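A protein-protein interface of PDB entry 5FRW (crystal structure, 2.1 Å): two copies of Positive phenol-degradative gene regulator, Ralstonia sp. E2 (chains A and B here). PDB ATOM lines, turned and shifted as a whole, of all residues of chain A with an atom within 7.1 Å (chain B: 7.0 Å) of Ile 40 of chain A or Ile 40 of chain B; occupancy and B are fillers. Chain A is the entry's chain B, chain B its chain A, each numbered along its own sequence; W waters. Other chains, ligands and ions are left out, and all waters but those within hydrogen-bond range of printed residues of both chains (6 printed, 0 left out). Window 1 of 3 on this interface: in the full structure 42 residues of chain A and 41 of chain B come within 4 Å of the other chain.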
ATOM      1  N   GLY A  30      15.464 -19.546  11.479  1.00  0.00           N
ATOM      2  CA  GLY A  30      15.319 -18.501  10.476  1.00  0.00           C
ATOM      3  C   GLY A  30      16.603 -18.223   9.714  1.00  0.00           C
ATOM      4  O   GLY A  30      16.971 -17.070   9.488  1.00  0.00           O
ATOM      5  N   ILE A  32      19.721 -19.649   6.626  1.00  0.00           N
ATOM      6  CA  ILE A  32      20.064 -20.411   5.449  1.00  0.00           C
ATOM      7  C   ILE A  32      21.569 -20.557   5.478  1.00  0.00           C
ATOM      8  O   ILE A  32      22.270 -19.569   5.727  1.00  0.00           O
ATOM      9  CB  ILE A  32      19.616 -19.713   4.136  1.00  0.00           C
ATOM     10  CG1 ILE A  32      18.077 -19.565   4.064  1.00  0.00           C
ATOM     11  CG2 ILE A  32      20.178 -20.446   2.934  1.00  0.00           C
ATOM     12  CD1 ILE A  32      17.593 -18.582   2.936  1.00  0.00           C
ATOM     13  N   ARG A  38      26.471 -18.273   6.720  1.00  0.00           N
ATOM     14  CA  ARG A  38      25.054 -17.919   6.724  1.00  0.00           C
ATOM     15  C   ARG A  38      24.728 -17.058   5.485  1.00  0.00           C
ATOM     16  O   ARG A  38      25.503 -16.164   5.114  1.00  0.00           O
ATOM     17  CB  ARG A  38      24.672 -17.192   8.013  1.00  0.00           C
ATOM     18  CG  ARG A  38      23.181 -16.937   8.118  1.00  0.00           C
ATOM     19  CD  ARG A  38      22.798 -16.260   9.407  1.00  0.00           C
ATOM     20  NE  ARG A  38      21.361 -16.011   9.418  1.00  0.00           N
ATOM     21  CZ  ARG A  38      20.669 -15.630  10.489  1.00  0.00           C
ATOM     22  NH1 ARG A  38      21.277 -15.449  11.661  1.00  0.00           N
ATOM     23  NH2 ARG A  38      19.361 -15.424  10.384  1.00  0.00           N
ATOM     24  N   MET A  39      23.601 -17.344   4.832  1.00  0.00           N
ATOM     25  CA  MET A  39      23.187 -16.599   3.621  1.00  0.00           C
ATOM     26  C   MET A  39      21.811 -15.985   3.796  1.00  0.00           C
ATOM     27  O   MET A  39      21.022 -16.489   4.571  1.00  0.00           O
ATOM     28  CB  MET A  39      23.153 -17.518   2.400  1.00  0.00           C
ATOM     29  CG  MET A  39      24.286 -18.580   2.366  1.00  0.00           C
ATOM     30  SD  MET A  39      25.827 -17.814   1.865  1.00  0.00           S
ATOM     31  CE  MET A  39      25.533 -17.457   0.152  1.00  0.00           C
ATOM     32  N   ILE A  40      21.495 -14.920   3.059  1.00  0.00           N
ATOM     33  CA  ILE A  40      20.099 -14.510   2.995  1.00  0.00           C
ATOM     34  C   ILE A  40      19.619 -14.503   1.549  1.00  0.00           C
ATOM     35  O   ILE A  40      20.413 -14.317   0.622  1.00  0.00           O
ATOM     36  CB  ILE A  40      19.858 -13.114   3.603  1.00  0.00           C
ATOM     37  CG1 ILE A  40      20.538 -12.030   2.765  1.00  0.00           C
ATOM     38  CG2 ILE A  40      20.336 -13.067   5.046  1.00  0.00           C
ATOM     39  CD1 ILE A  40      20.108 -10.642   3.151  1.00  0.00           C
ATOM     40  N   LEU A  41      18.329 -14.719   1.344  1.00  0.00           N
ATOM     41  CA  LEU A  41      17.759 -14.467   0.041  1.00  0.00           C
ATOM     42  C   LEU A  41      17.431 -12.989  -0.041  1.00  0.00           C
ATOM     43  O   LEU A  41      16.648 -12.489   0.754  1.00  0.00           O
ATOM     44  CB  LEU A  41      16.504 -15.297  -0.185  1.00  0.00           C
ATOM     45  CG  LEU A  41      16.778 -16.735  -0.571  1.00  0.00           C
ATOM     46  CD1 LEU A  41      15.540 -17.561  -0.441  1.00  0.00           C
ATOM     47  CD2 LEU A  41      17.274 -16.730  -2.013  1.00  0.00           C
ATOM     48  N   LEU A  42      18.022 -12.296  -1.003  1.00  0.00           N
ATOM     49  CA  LEU A  42      17.777 -10.869  -1.154  1.00  0.00           C
ATOM     50  C   LEU A  42      17.228 -10.581  -2.539  1.00  0.00           C
ATOM     51  O   LEU A  42      17.663 -11.193  -3.511  1.00  0.00           O
ATOM     52  CB  LEU A  42      19.067 -10.087  -0.908  1.00  0.00           C
ATOM     53  CG  LEU A  42      19.066  -8.554  -0.959  1.00  0.00           C
ATOM     54  CD1 LEU A  42      18.149  -7.951   0.125  1.00  0.00           C
ATOM     55  CD2 LEU A  42      20.502  -8.066  -0.800  1.00  0.00           C
ATOM     56  N   HIS A  43      16.272  -9.656  -2.625  1.00  0.00           N
ATOM     57  CA  HIS A  43      15.655  -9.289  -3.891  1.00  0.00           C
ATOM     58  C   HIS A  43      16.659  -8.533  -4.709  1.00  0.00           C
ATOM     59  O   HIS A  43      17.251  -7.595  -4.197  1.00  0.00           O
ATOM     60  CB  HIS A  43      14.407  -8.399  -3.685  1.00  0.00           C
ATOM     61  CG  HIS A  43      13.403  -8.973  -2.742  1.00  0.00           C
ATOM     62  ND1 HIS A  43      13.624  -9.049  -1.384  1.00  0.00           N
ATOM     63  CD2 HIS A  43      12.180  -9.514  -2.960  1.00  0.00           C
ATOM     64  CE1 HIS A  43      12.580  -9.615  -0.804  1.00  0.00           C
ATOM     65  NE2 HIS A  43      11.689  -9.904  -1.737  1.00  0.00           N
ATOM     66  N   THR A  44      16.849  -8.897  -5.972  1.00  0.00           N
ATOM     67  CA  THR A  44      17.754  -8.099  -6.797  1.00  0.00           C
ATOM     68  C   THR A  44      17.257  -6.647  -6.911  1.00  0.00           C
ATOM     69  O   THR A  44      18.056  -5.703  -6.995  1.00  0.00           O
ATOM     70  CB  THR A  44      17.929  -8.691  -8.219  1.00  0.00           C
ATOM     71  OG1 THR A  44      16.653  -8.853  -8.834  1.00  0.00           O
ATOM     72  CG2 THR A  44      18.583 -10.043  -8.131  1.00  0.00           C
ATOM     73  N   LEU A  47      18.717  -4.717  -4.017  1.00  0.00           N
ATOM     74  CA  LEU A  47      20.141  -4.516  -4.228  1.00  0.00           C
ATOM     75  C   LEU A  47      20.346  -3.430  -5.278  1.00  0.00           C
ATOM     76  O   LEU A  47      21.214  -2.568  -5.146  1.00  0.00           O
ATOM     77  CB  LEU A  47      20.817  -5.832  -4.638  1.00  0.00           C
ATOM     78  CG  LEU A  47      22.294  -5.949  -4.277  1.00  0.00           C
ATOM     79  CD1 LEU A  47      22.509  -5.617  -2.816  1.00  0.00           C
ATOM     80  CD2 LEU A  47      22.847  -7.350  -4.570  1.00  0.00           C
ATOM     81  N   ILE A 104      24.535 -21.524  -8.364  1.00  0.00           N
ATOM     82  CA  ILE A 104      23.582 -21.954  -7.342  1.00  0.00           C
ATOM     83  C   ILE A 104      23.004 -20.747  -6.569  1.00  0.00           C
ATOM     84  O   ILE A 104      21.826 -20.716  -6.213  1.00  0.00           O
ATOM     85  CB  ILE A 104      24.258 -22.965  -6.388  1.00  0.00           C
ATOM     86  CG1 ILE A 104      24.448 -24.305  -7.108  1.00  0.00           C
ATOM     87  CG2 ILE A 104      23.429 -23.195  -5.160  1.00  0.00           C
ATOM     88  CD1 ILE A 104      25.459 -25.259  -6.434  1.00  0.00           C
ATOM     89  N   GLU A 105      23.829 -19.735  -6.355  1.00  0.00           N
ATOM     90  CA  GLU A 105      23.418 -18.544  -5.619  1.00  0.00           C
ATOM     91  C   GLU A 105      22.462 -17.651  -6.421  1.00  0.00           C
ATOM     92  O   GLU A 105      21.992 -16.629  -5.913  1.00  0.00           O
ATOM     93  CB  GLU A 105      24.658 -17.764  -5.174  1.00  0.00           C
ATOM     94  CG  GLU A 105      25.356 -18.489  -3.972  1.00  0.00           C
ATOM     95  CD  GLU A 105      26.862 -18.225  -3.809  1.00  0.00           C
ATOM     96  OE1 GLU A 105      27.398 -17.243  -4.370  1.00  0.00           O
ATOM     97  OE2 GLU A 105      27.524 -19.014  -3.087  1.00  0.00           O
ATOM     98  N   GLY A 106      22.165 -18.055  -7.656  1.00  0.00           N
ATOM     99  CA  GLY A 106      21.277 -17.301  -8.538  1.00  0.00           C
ATOM    100  C   GLY A 106      21.873 -16.002  -9.045  1.00  0.00           C
ATOM    101  O   GLY A 106      21.146 -15.132  -9.517  1.00  0.00           O
ATOM    102  N   VAL A 107      23.197 -15.862  -8.955  1.00  0.00           N
ATOM    103  CA  VAL A 107      23.858 -14.611  -9.346  1.00  0.00           C
ATOM    104  C   VAL A 107      24.014 -14.515 -10.876  1.00  0.00           C
ATOM    105  O   VAL A 107      23.700 -13.487 -11.486  1.00  0.00           O
ATOM    106  CB  VAL A 107      25.242 -14.468  -8.672  1.00  0.00           C
ATOM    107  CG1 VAL A 107      25.986 -13.255  -9.231  1.00  0.00           C
ATOM    108  CG2 VAL A 107      25.095 -14.368  -7.139  1.00  0.00           C
ATOM    109  N   VAL A 108      24.467 -15.603 -11.485  1.00  0.00           N
ATOM    110  CA  VAL A 108      24.750 -15.643 -12.918  1.00  0.00           C
ATOM    111  C   VAL A 108      24.909 -17.098 -13.325  1.00  0.00           C
ATOM    112  O   VAL A 108      25.336 -17.921 -12.521  1.00  0.00           O
ATOM    113  CB  VAL A 108      26.023 -14.851 -13.268  1.00  0.00           C
ATOM    114  CG1 VAL A 108      27.254 -15.458 -12.562  1.00  0.00           C
ATOM    115  CG2 VAL A 108      26.252 -14.823 -14.775  1.00  0.00           C
ATOM    116  N   PHE A 134      22.661 -11.083 -13.066  1.00  0.00           N
ATOM    117  CA  PHE A 134      21.638 -10.263 -12.397  1.00  0.00           C
ATOM    118  C   PHE A 134      22.115  -8.824 -12.376  1.00  0.00           C
ATOM    119  O   PHE A 134      21.324  -7.894 -12.472  1.00  0.00           O
ATOM    120  CB  PHE A 134      21.338 -10.737 -10.964  1.00  0.00           C
ATOM    121  CG  PHE A 134      22.164 -10.039  -9.890  1.00  0.00           C
ATOM    122  CD1 PHE A 134      21.732  -8.842  -9.319  1.00  0.00           C
ATOM    123  CD2 PHE A 134      23.343 -10.596  -9.438  1.00  0.00           C
ATOM    124  CE1 PHE A 134      22.484  -8.196  -8.333  1.00  0.00           C
ATOM    125  CE2 PHE A 134      24.103  -9.965  -8.452  1.00  0.00           C
ATOM    126  CZ  PHE A 134      23.662  -8.751  -7.897  1.00  0.00           C
ATOM    127  N   GLU A 135      23.426  -8.654 -12.242  1.00  0.00           N
ATOM    128  CA  GLU A 135      23.990  -7.328 -12.053  1.00  0.00           C
ATOM    129  C   GLU A 135      23.828  -6.465 -13.288  1.00  0.00           C
ATOM    130  O   GLU A 135      23.262  -5.370 -13.216  1.00  0.00           O
ATOM    131  CB  GLU A 135      25.462  -7.423 -11.675  1.00  0.00           C
ATOM    132  CG  GLU A 135      25.734  -6.941 -10.277  1.00  0.00           C
ATOM    133  CD  GLU A 135      27.204  -6.711 -10.016  1.00  0.00           C
ATOM    134  OE1 GLU A 135      28.029  -7.633 -10.293  1.00  0.00           O
ATOM    135  OE2 GLU A 135      27.535  -5.600  -9.530  1.00  0.00           O
ATOM    136  N   MET A 153      30.119  -6.672  -8.736  1.00  0.00           N
ATOM    137  CA  MET A 153      30.083  -7.679  -7.672  1.00  0.00           C
ATOM    138  C   MET A 153      30.425  -9.073  -8.192  1.00  0.00           C
ATOM    139  O   MET A 153      31.071  -9.873  -7.493  1.00  0.00           O
ATOM    140  CB  MET A 153      28.703  -7.699  -7.015  1.00  0.00           C
ATOM    141  CG  MET A 153      28.652  -8.446  -5.689  1.00  0.00           C
ATOM    142  SD  MET A 153      26.949  -8.525  -5.050  1.00  0.00           S
ATOM    143  CE  MET A 153      26.178  -7.304  -6.118  1.00  0.00           C
ATOM    144  N   GLY B  30      20.826 -20.461 -13.651  1.00  0.00           N
ATOM    145  CA  GLY B  30      21.520 -19.705 -12.618  1.00  0.00           C
ATOM    146  C   GLY B  30      20.655 -18.607 -12.004  1.00  0.00           C
ATOM    147  O   GLY B  30      21.120 -17.490 -11.766  1.00  0.00           O
ATOM    148  N   ILE B  32      17.193 -17.591  -9.183  1.00  0.00           N
ATOM    149  CA  ILE B  32      16.246 -17.898  -8.131  1.00  0.00           C
ATOM    150  C   ILE B  32      15.094 -16.890  -8.195  1.00  0.00           C
ATOM    151  O   ILE B  32      15.322 -15.676  -8.248  1.00  0.00           O
ATOM    152  CB  ILE B  32      16.901 -17.836  -6.734  1.00  0.00           C
ATOM    153  CG1 ILE B  32      18.077 -18.809  -6.642  1.00  0.00           C
ATOM    154  CG2 ILE B  32      15.865 -18.097  -5.660  1.00  0.00           C
ATOM    155  CD1 ILE B  32      18.929 -18.559  -5.417  1.00  0.00           C
ATOM    156  N   ARG B  38      13.099 -11.620  -8.824  1.00  0.00           N
ATOM    157  CA  ARG B  38      14.354 -12.363  -8.881  1.00  0.00           C
ATOM    158  C   ARG B  38      15.154 -12.129  -7.589  1.00  0.00           C
ATOM    159  O   ARG B  38      15.242 -10.995  -7.106  1.00  0.00           O
ATOM    160  CB  ARG B  38      15.184 -11.966 -10.099  1.00  0.00           C
ATOM    161  CG  ARG B  38      16.520 -12.754 -10.182  1.00  0.00           C
ATOM    162  CD  ARG B  38      17.255 -12.539 -11.495  1.00  0.00           C
ATOM    163  NE  ARG B  38      18.500 -13.296 -11.512  1.00  0.00           N
ATOM    164  CZ  ARG B  38      19.367 -13.319 -12.520  1.00  0.00           C
ATOM    165  NH1 ARG B  38      19.148 -12.628 -13.628  1.00  0.00           N
ATOM    166  NH2 ARG B  38      20.467 -14.044 -12.415  1.00  0.00           N
ATOM    167  N   MET B  39      15.723 -13.205  -7.049  1.00  0.00           N
ATOM    168  CA  MET B  39      16.494 -13.192  -5.794  1.00  0.00           C
ATOM    169  C   MET B  39      17.928 -13.687  -6.026  1.00  0.00           C
ATOM    170  O   MET B  39      18.162 -14.463  -6.960  1.00  0.00           O
ATOM    171  CB  MET B  39      15.842 -14.103  -4.748  1.00  0.00           C
ATOM    172  CG  MET B  39      14.319 -14.047  -4.741  1.00  0.00           C
ATOM    173  SD  MET B  39      13.761 -12.531  -3.974  1.00  0.00           S
ATOM    174  CE  MET B  39      14.102 -12.863  -2.246  1.00  0.00           C
ATOM    175  N   ILE B  40      18.870 -13.266  -5.176  1.00  0.00           N
ATOM    176  CA  ILE B  40      20.161 -13.958  -5.083  1.00  0.00           C
ATOM    177  C   ILE B  40      20.385 -14.439  -3.664  1.00  0.00           C
ATOM    178  O   ILE B  40      19.825 -13.876  -2.716  1.00  0.00           O
ATOM    179  CB  ILE B  40      21.384 -13.080  -5.494  1.00  0.00           C
ATOM    180  CG1 ILE B  40      21.610 -11.928  -4.522  1.00  0.00           C
ATOM    181  CG2 ILE B  40      21.271 -12.585  -6.924  1.00  0.00           C
ATOM    182  CD1 ILE B  40      22.838 -11.120  -4.847  1.00  0.00           C
ATOM    183  N   LEU B  41      21.202 -15.481  -3.524  1.00  0.00           N
ATOM    184  CA  LEU B  41      21.695 -15.896  -2.220  1.00  0.00           C
ATOM    185  C   LEU B  41      22.954 -15.095  -1.942  1.00  0.00           C
ATOM    186  O   LEU B  41      23.917 -15.175  -2.699  1.00  0.00           O
ATOM    187  CB  LEU B  41      21.993 -17.414  -2.177  1.00  0.00           C
ATOM    188  CG  LEU B  41      20.771 -18.308  -1.969  1.00  0.00           C
ATOM    189  CD1 LEU B  41      21.054 -19.790  -2.249  1.00  0.00           C
ATOM    190  CD2 LEU B  41      20.302 -18.126  -0.559  1.00  0.00           C
ATOM    191  N   LEU B  42      22.965 -14.346  -0.852  1.00  0.00           N
ATOM    192  CA  LEU B  42      24.114 -13.502  -0.550  1.00  0.00           C
ATOM    193  C   LEU B  42      24.696 -13.806   0.832  1.00  0.00           C
ATOM    194  O   LEU B  42      23.963 -13.895   1.811  1.00  0.00           O
ATOM    195  CB  LEU B  42      23.712 -12.023  -0.637  1.00  0.00           C
ATOM    196  CG  LEU B  42      24.781 -10.942  -0.484  1.00  0.00           C
ATOM    197  CD1 LEU B  42      25.806 -11.057  -1.599  1.00  0.00           C
ATOM    198  CD2 LEU B  42      24.079  -9.579  -0.546  1.00  0.00           C
ATOM    199  N   HIS B  43      26.021 -13.931   0.901  1.00  0.00           N
ATOM    200  CA  HIS B  43      26.713 -14.175   2.164  1.00  0.00           C
ATOM    201  C   HIS B  43      26.493 -12.998   3.117  1.00  0.00           C
ATOM    202  O   HIS B  43      26.700 -11.835   2.745  1.00  0.00           O
ATOM    203  CB  HIS B  43      28.209 -14.402   1.928  1.00  0.00           C
ATOM    204  CG  HIS B  43      28.509 -15.432   0.878  1.00  0.00           C
ATOM    205  ND1 HIS B  43      28.256 -15.230  -0.462  1.00  0.00           N
ATOM    206  CD2 HIS B  43      29.048 -16.675   0.977  1.00  0.00           C
ATOM    207  CE1 HIS B  43      28.633 -16.300  -1.146  1.00  0.00           C
ATOM    208  NE2 HIS B  43      29.108 -17.191  -0.296  1.00  0.00           N
ATOM    209  N   THR B  44      26.033 -13.283   4.329  1.00  0.00           N
ATOM    210  CA  THR B  44      25.860 -12.215   5.309  1.00  0.00           C
ATOM    211  C   THR B  44      27.201 -11.516   5.570  1.00  0.00           C
ATOM    212  O   THR B  44      27.255 -10.310   5.841  1.00  0.00           O
ATOM    213  CB  THR B  44      25.295 -12.756   6.621  1.00  0.00           C
ATOM    214  OG1 THR B  44      26.166 -13.789   7.109  1.00  0.00           O
ATOM    215  CG2 THR B  44      23.913 -13.344   6.387  1.00  0.00           C
ATOM    216  N   LEU B  47      27.612  -8.776   2.994  1.00  0.00           N
ATOM    217  CA  LEU B  47      26.765  -7.652   3.376  1.00  0.00           C
ATOM    218  C   LEU B  47      27.356  -6.949   4.611  1.00  0.00           C
ATOM    219  O   LEU B  47      27.281  -5.731   4.730  1.00  0.00           O
ATOM    220  CB  LEU B  47      25.332  -8.112   3.657  1.00  0.00           C
ATOM    221  CG  LEU B  47      24.240  -7.833   2.606  1.00  0.00           C
ATOM    222  CD1 LEU B  47      22.873  -8.222   3.130  1.00  0.00           C
ATOM    223  CD2 LEU B  47      24.229  -6.385   2.149  1.00  0.00           C
ATOM    224  N   ILE B 104      11.826 -17.347   5.638  1.00  0.00           N
ATOM    225  CA  ILE B 104      12.228 -18.159   4.484  1.00  0.00           C
ATOM    226  C   ILE B 104      13.434 -17.565   3.774  1.00  0.00           C
ATOM    227  O   ILE B 104      14.274 -18.283   3.226  1.00  0.00           O
ATOM    228  CB  ILE B 104      11.079 -18.310   3.479  1.00  0.00           C
ATOM    229  CG1 ILE B 104       9.898 -19.005   4.144  1.00  0.00           C
ATOM    230  CG2 ILE B 104      11.497 -19.148   2.300  1.00  0.00           C
ATOM    231  CD1 ILE B 104       8.644 -18.980   3.293  1.00  0.00           C
ATOM    232  N   GLU B 105      13.542 -16.249   3.818  1.00  0.00           N
ATOM    233  CA  GLU B 105      14.666 -15.558   3.217  1.00  0.00           C
ATOM    234  C   GLU B 105      15.880 -15.581   4.138  1.00  0.00           C
ATOM    235  O   GLU B 105      16.943 -15.055   3.778  1.00  0.00           O
ATOM    236  CB  GLU B 105      14.281 -14.110   2.854  1.00  0.00           C
ATOM    237  CG  GLU B 105      13.224 -14.067   1.769  1.00  0.00           C
ATOM    238  CD  GLU B 105      12.528 -12.714   1.646  1.00  0.00           C
ATOM    239  OE1 GLU B 105      12.993 -11.717   2.235  1.00  0.00           O
ATOM    240  OE2 GLU B 105      11.491 -12.667   0.971  1.00  0.00           O
ATOM    241  N   GLY B 106      15.725 -16.222   5.304  1.00  0.00           N
ATOM    242  CA  GLY B 106      16.832 -16.468   6.217  1.00  0.00           C
ATOM    243  C   GLY B 106      17.325 -15.213   6.910  1.00  0.00           C
ATOM    244  O   GLY B 106      18.462 -15.121   7.381  1.00  0.00           O
ATOM    245  N   VAL B 107      16.451 -14.228   6.982  1.00  0.00           N
ATOM    246  CA  VAL B 107      16.809 -12.951   7.571  1.00  0.00           C
ATOM    247  C   VAL B 107      16.707 -13.033   9.091  1.00  0.00           C
ATOM    248  O   VAL B 107      17.619 -12.622   9.792  1.00  0.00           O
ATOM    249  CB  VAL B 107      15.911 -11.814   7.001  1.00  0.00           C
ATOM    250  CG1 VAL B 107      16.210 -10.483   7.670  1.00  0.00           C
ATOM    251  CG2 VAL B 107      16.112 -11.720   5.480  1.00  0.00           C
ATOM    252  N   VAL B 108      15.608 -13.604   9.575  1.00  0.00           N
ATOM    253  CA  VAL B 108      15.278 -13.629  10.989  1.00  0.00           C
ATOM    254  C   VAL B 108      14.146 -14.627  11.223  1.00  0.00           C
ATOM    255  O   VAL B 108      13.327 -14.865  10.335  1.00  0.00           O
ATOM    256  CB  VAL B 108      14.896 -12.185  11.477  1.00  0.00           C
ATOM    257  CG1 VAL B 108      13.626 -11.689  10.791  1.00  0.00           C
ATOM    258  CG2 VAL B 108      14.719 -12.129  12.989  1.00  0.00           C
ATOM    259  N   PHE B 134      20.009 -11.945  11.468  1.00  0.00           N
ATOM    260  CA  PHE B 134      21.311 -11.941  10.810  1.00  0.00           C
ATOM    261  C   PHE B 134      21.953 -10.584  11.006  1.00  0.00           C
ATOM    262  O   PHE B 134      23.169 -10.450  11.072  1.00  0.00           O
ATOM    263  CB  PHE B 134      21.198 -12.243   9.319  1.00  0.00           C
ATOM    264  CG  PHE B 134      21.135 -11.011   8.445  1.00  0.00           C
ATOM    265  CD1 PHE B 134      22.299 -10.417   7.973  1.00  0.00           C
ATOM    266  CD2 PHE B 134      19.925 -10.461   8.086  1.00  0.00           C
ATOM    267  CE1 PHE B 134      22.252  -9.292   7.177  1.00  0.00           C
ATOM    268  CE2 PHE B 134      19.861  -9.323   7.281  1.00  0.00           C
ATOM    269  CZ  PHE B 134      21.028  -8.744   6.821  1.00  0.00           C
ATOM    270  N   MET B 153      18.004  -2.921   8.020  1.00  0.00           N
ATOM    271  CA  MET B 153      17.336  -3.550   6.899  1.00  0.00           C
ATOM    272  C   MET B 153      16.111  -4.319   7.357  1.00  0.00           C
ATOM    273  O   MET B 153      15.084  -4.293   6.685  1.00  0.00           O
ATOM    274  CB  MET B 153      18.278  -4.486   6.173  1.00  0.00           C
ATOM    275  CG  MET B 153      17.798  -4.889   4.785  1.00  0.00           C
ATOM    276  SD  MET B 153      18.958  -6.135   4.087  1.00  0.00           S
ATOM    277  CE  MET B 153      20.512  -5.615   4.778  1.00  0.00           C
HETATM  278  O   HOH W   1      26.467 -14.456  -3.684  1.00  0.00           O
HETATM  279  O   HOH W   2      18.669 -15.141  -9.355  1.00  0.00           O
HETATM  280  O   HOH W   3      15.308 -10.416   1.913  1.00  0.00           O
HETATM  281  O   HOH W   4      20.281 -16.828   6.990  1.00  0.00           O
HETATM  282  O   HOH W   5      28.279 -15.285   5.371  1.00  0.00           O
HETATM  283  O   HOH W   6      13.785  -8.584  -7.193  1.00  0.00           O
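His 43 of chain B touches Arg 38 of chain A. Met 39 of chain A touches Leu 42 of chain B (CA to O, 3.3 Å). CD2 of His 43 of chain B touches SD of Met 39 of chain A (3.5 Å). CA of Ile 40 of chain A touches O of Glu 105 of chain B, 3.3 Å away. Leu 41 of chain A touches Leu 41 of chain B (CD2 to CD2, 3.6 Å). SD of Met 39 of chain B touches CD2 of His 43 of chain A (3.6 Å). Thr 44 of chain A touches Ile 40 of chain B. OE2 of Glu 105 of chain A touches CE1 of His 43 of chain B (3.5 Å). CB of Phe 134 of chain A touches CZ of Arg 38 of chain B, 3.6 Å away.
Water W4 lies within hydrogen-bond range of the backbone carbonyl oxygen (O) of Gly 106 of chain B (2.5 Å), the backbone carbonyl oxygen (O) of Met 39 of chain A (2.6 Å), the guanidinium group (NE) of Arg 38 of chain A (2.8 Å) and the backbone NH (N) of Ile 32 of chain A (2.9 Å). Water W6 lies within hydrogen-bond range of O of Arg 38 of chain B (2.8 Å) and N of Thr 44 of chain A (3.3 Å). Water W5 lies within hydrogen-bond range of O of Arg 38 of chain A (2.9 Å) and OG1 of Thr 44 of chain B (3.1 Å).
Of the 17 printed residues of chain B, 16 touch a printed residue of chain A. Hydrophobic or aromatic side chains of chain B within 4 Å of the printed part of chain A: Ile 32, Met 39, Ile 40, Leu 41, Leu 42, His 43, Leu 47 and Phe 134. Among the printed residues, no Asp or Glu carboxylate lies within 4 Å of a Lys or Arg side-chain nitrogen of the other chain.
The backbone carbonyl oxygen (O) of Glu 105 of chain A lies within hydrogen-bond range of the backbone NH (N) of Leu 41 of chain B. O of Gly 30 of chain B lies close to O of Gly 106 of chain A, at 3.3 Å. The guanidinium group of Arg 38 of chain B lies within hydrogen-bond range of the backbone carbonyl oxygen of Gly 106 of chain A. N of Leu 42 of chain B is in hydrogen-bond range of O of Ile 40 of chain A (2.9 Å). O of Val 107 of chain B sits at hydrogen-bond distance from NH2 of Arg 38 of chain A (3.4 Å). The backbone carbonyl oxygen (O) of Leu 42 of chain A is in hydrogen-bond range of the backbone NH (N) of Ile 40 of chain B (2.9 Å). The backbone carbonyl oxygen (O) of Arg 38 of chain B lies within hydrogen-bond range of the backbone NH (N) of Thr 44 of chain A, at 2.9 Å. The guanidinium group (NH2) of Arg 38 of chain B sits at hydrogen-bond distance from the backbone carbonyl oxygen (O) of Val 107 of chain A. The backbone NH (N) of Thr 44 of chain B is in hydrogen-bond range of the backbone carbonyl oxygen (O) of Arg 38 of chain A (3.0 Å). O of Glu 105 of chain B is in hydrogen-bond range of N of Leu 41 of chain A (2.8 Å). The backbone carbonyl oxygen (O) of Gly 30 of chain A sits close to the backbone carbonyl oxygen (O) of Gly 106 of chain B (3.2 Å). The backbone carbonyl oxygen (O) of Ile 40 of chain B lies close to the backbone carbonyl oxygen (O) of Ile 40 of chain A, 3.4 Å away. The backbone carbonyl oxygen of Gly 106 of chain B lies within hydrogen-bond range of the guanidinium group of Arg 38 of chain A, at 3.1 Å.
The backbone NH (N) of Phe 134 of chain A lies within hydrogen-bond range of the backbone carbonyl oxygen (O) of Val 107 of chain A, 3.1 Å away. O of Gly 30 of chain A sits at hydrogen-bond distance from NH2 of Arg 38 of chain A. O of Ile 32 of chain B sits at hydrogen-bond distance from N of Met 39 of chain B, 2.8 Å away. The backbone NH (N) of Phe 134 of chain B is in hydrogen-bond range of the backbone carbonyl oxygen (O) of Val 107 of chain B. The backbone carbonyl oxygen (O) of Ile 32 of chain A is in hydrogen-bond range of the backbone NH (N) of Met 39 of chain A, at 2.7 Å.
Of chain B, only Ile 40, Leu 41, Leu 42, Thr 44, Leu 47, Glu 105 and Gly 106 come within 4 Å of Ile 40 of chain A. Of the printed residues of chain A, Ile 40 of chain B touches Ile 40, Leu 41, Leu 42, Thr 44, Leu 47, Glu 105, Gly 106 and Phe 134. Printed residues of chain A within 4 Å of Val 108 of chain B: Gly 30. Printed residues of chain A within 4 Å of Leu 41 of chain B: Met 39 (3.99 Å), Ile 40 (3.5 Å), Leu 41 (3.6 Å) and Glu 105 (2.8 Å). Printed residues of chain A within 4 Å of Leu 42 of chain B: Met 39, Ile 40 and Leu 42. Glu 135 of chain A touches none of the printed residues of chain B. Met 153 of chain A touches none of the printed residues of chain B. The nearest residue of chain A that does not touch Ile 40 of chain B is Val 107 of chain A (4.1 Å). The nearest printed residue of chain A that does not touch Gly 30 of chain B is Glu 105 of chain A (5.5 Å).
Ile 40 of chain A touches Leu 41 of chain B, and with the chains exchanged Leu 41 of chain A touches Ile 40 of chain B. His 43 of chain A touches Glu 105 of chain B, and with the chains exchanged Glu 105 of chain A touches His 43 of chain B. Positions printed for both chains: 30, 32, 38, 39, 40, 41, 42, 43, 44, 47, 104, 105, 106, 107, 108, 134 and 153. Of the 50 pairs that touch across the chains among the printed residues, 47 have their exchanged pair printed and touching as well.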
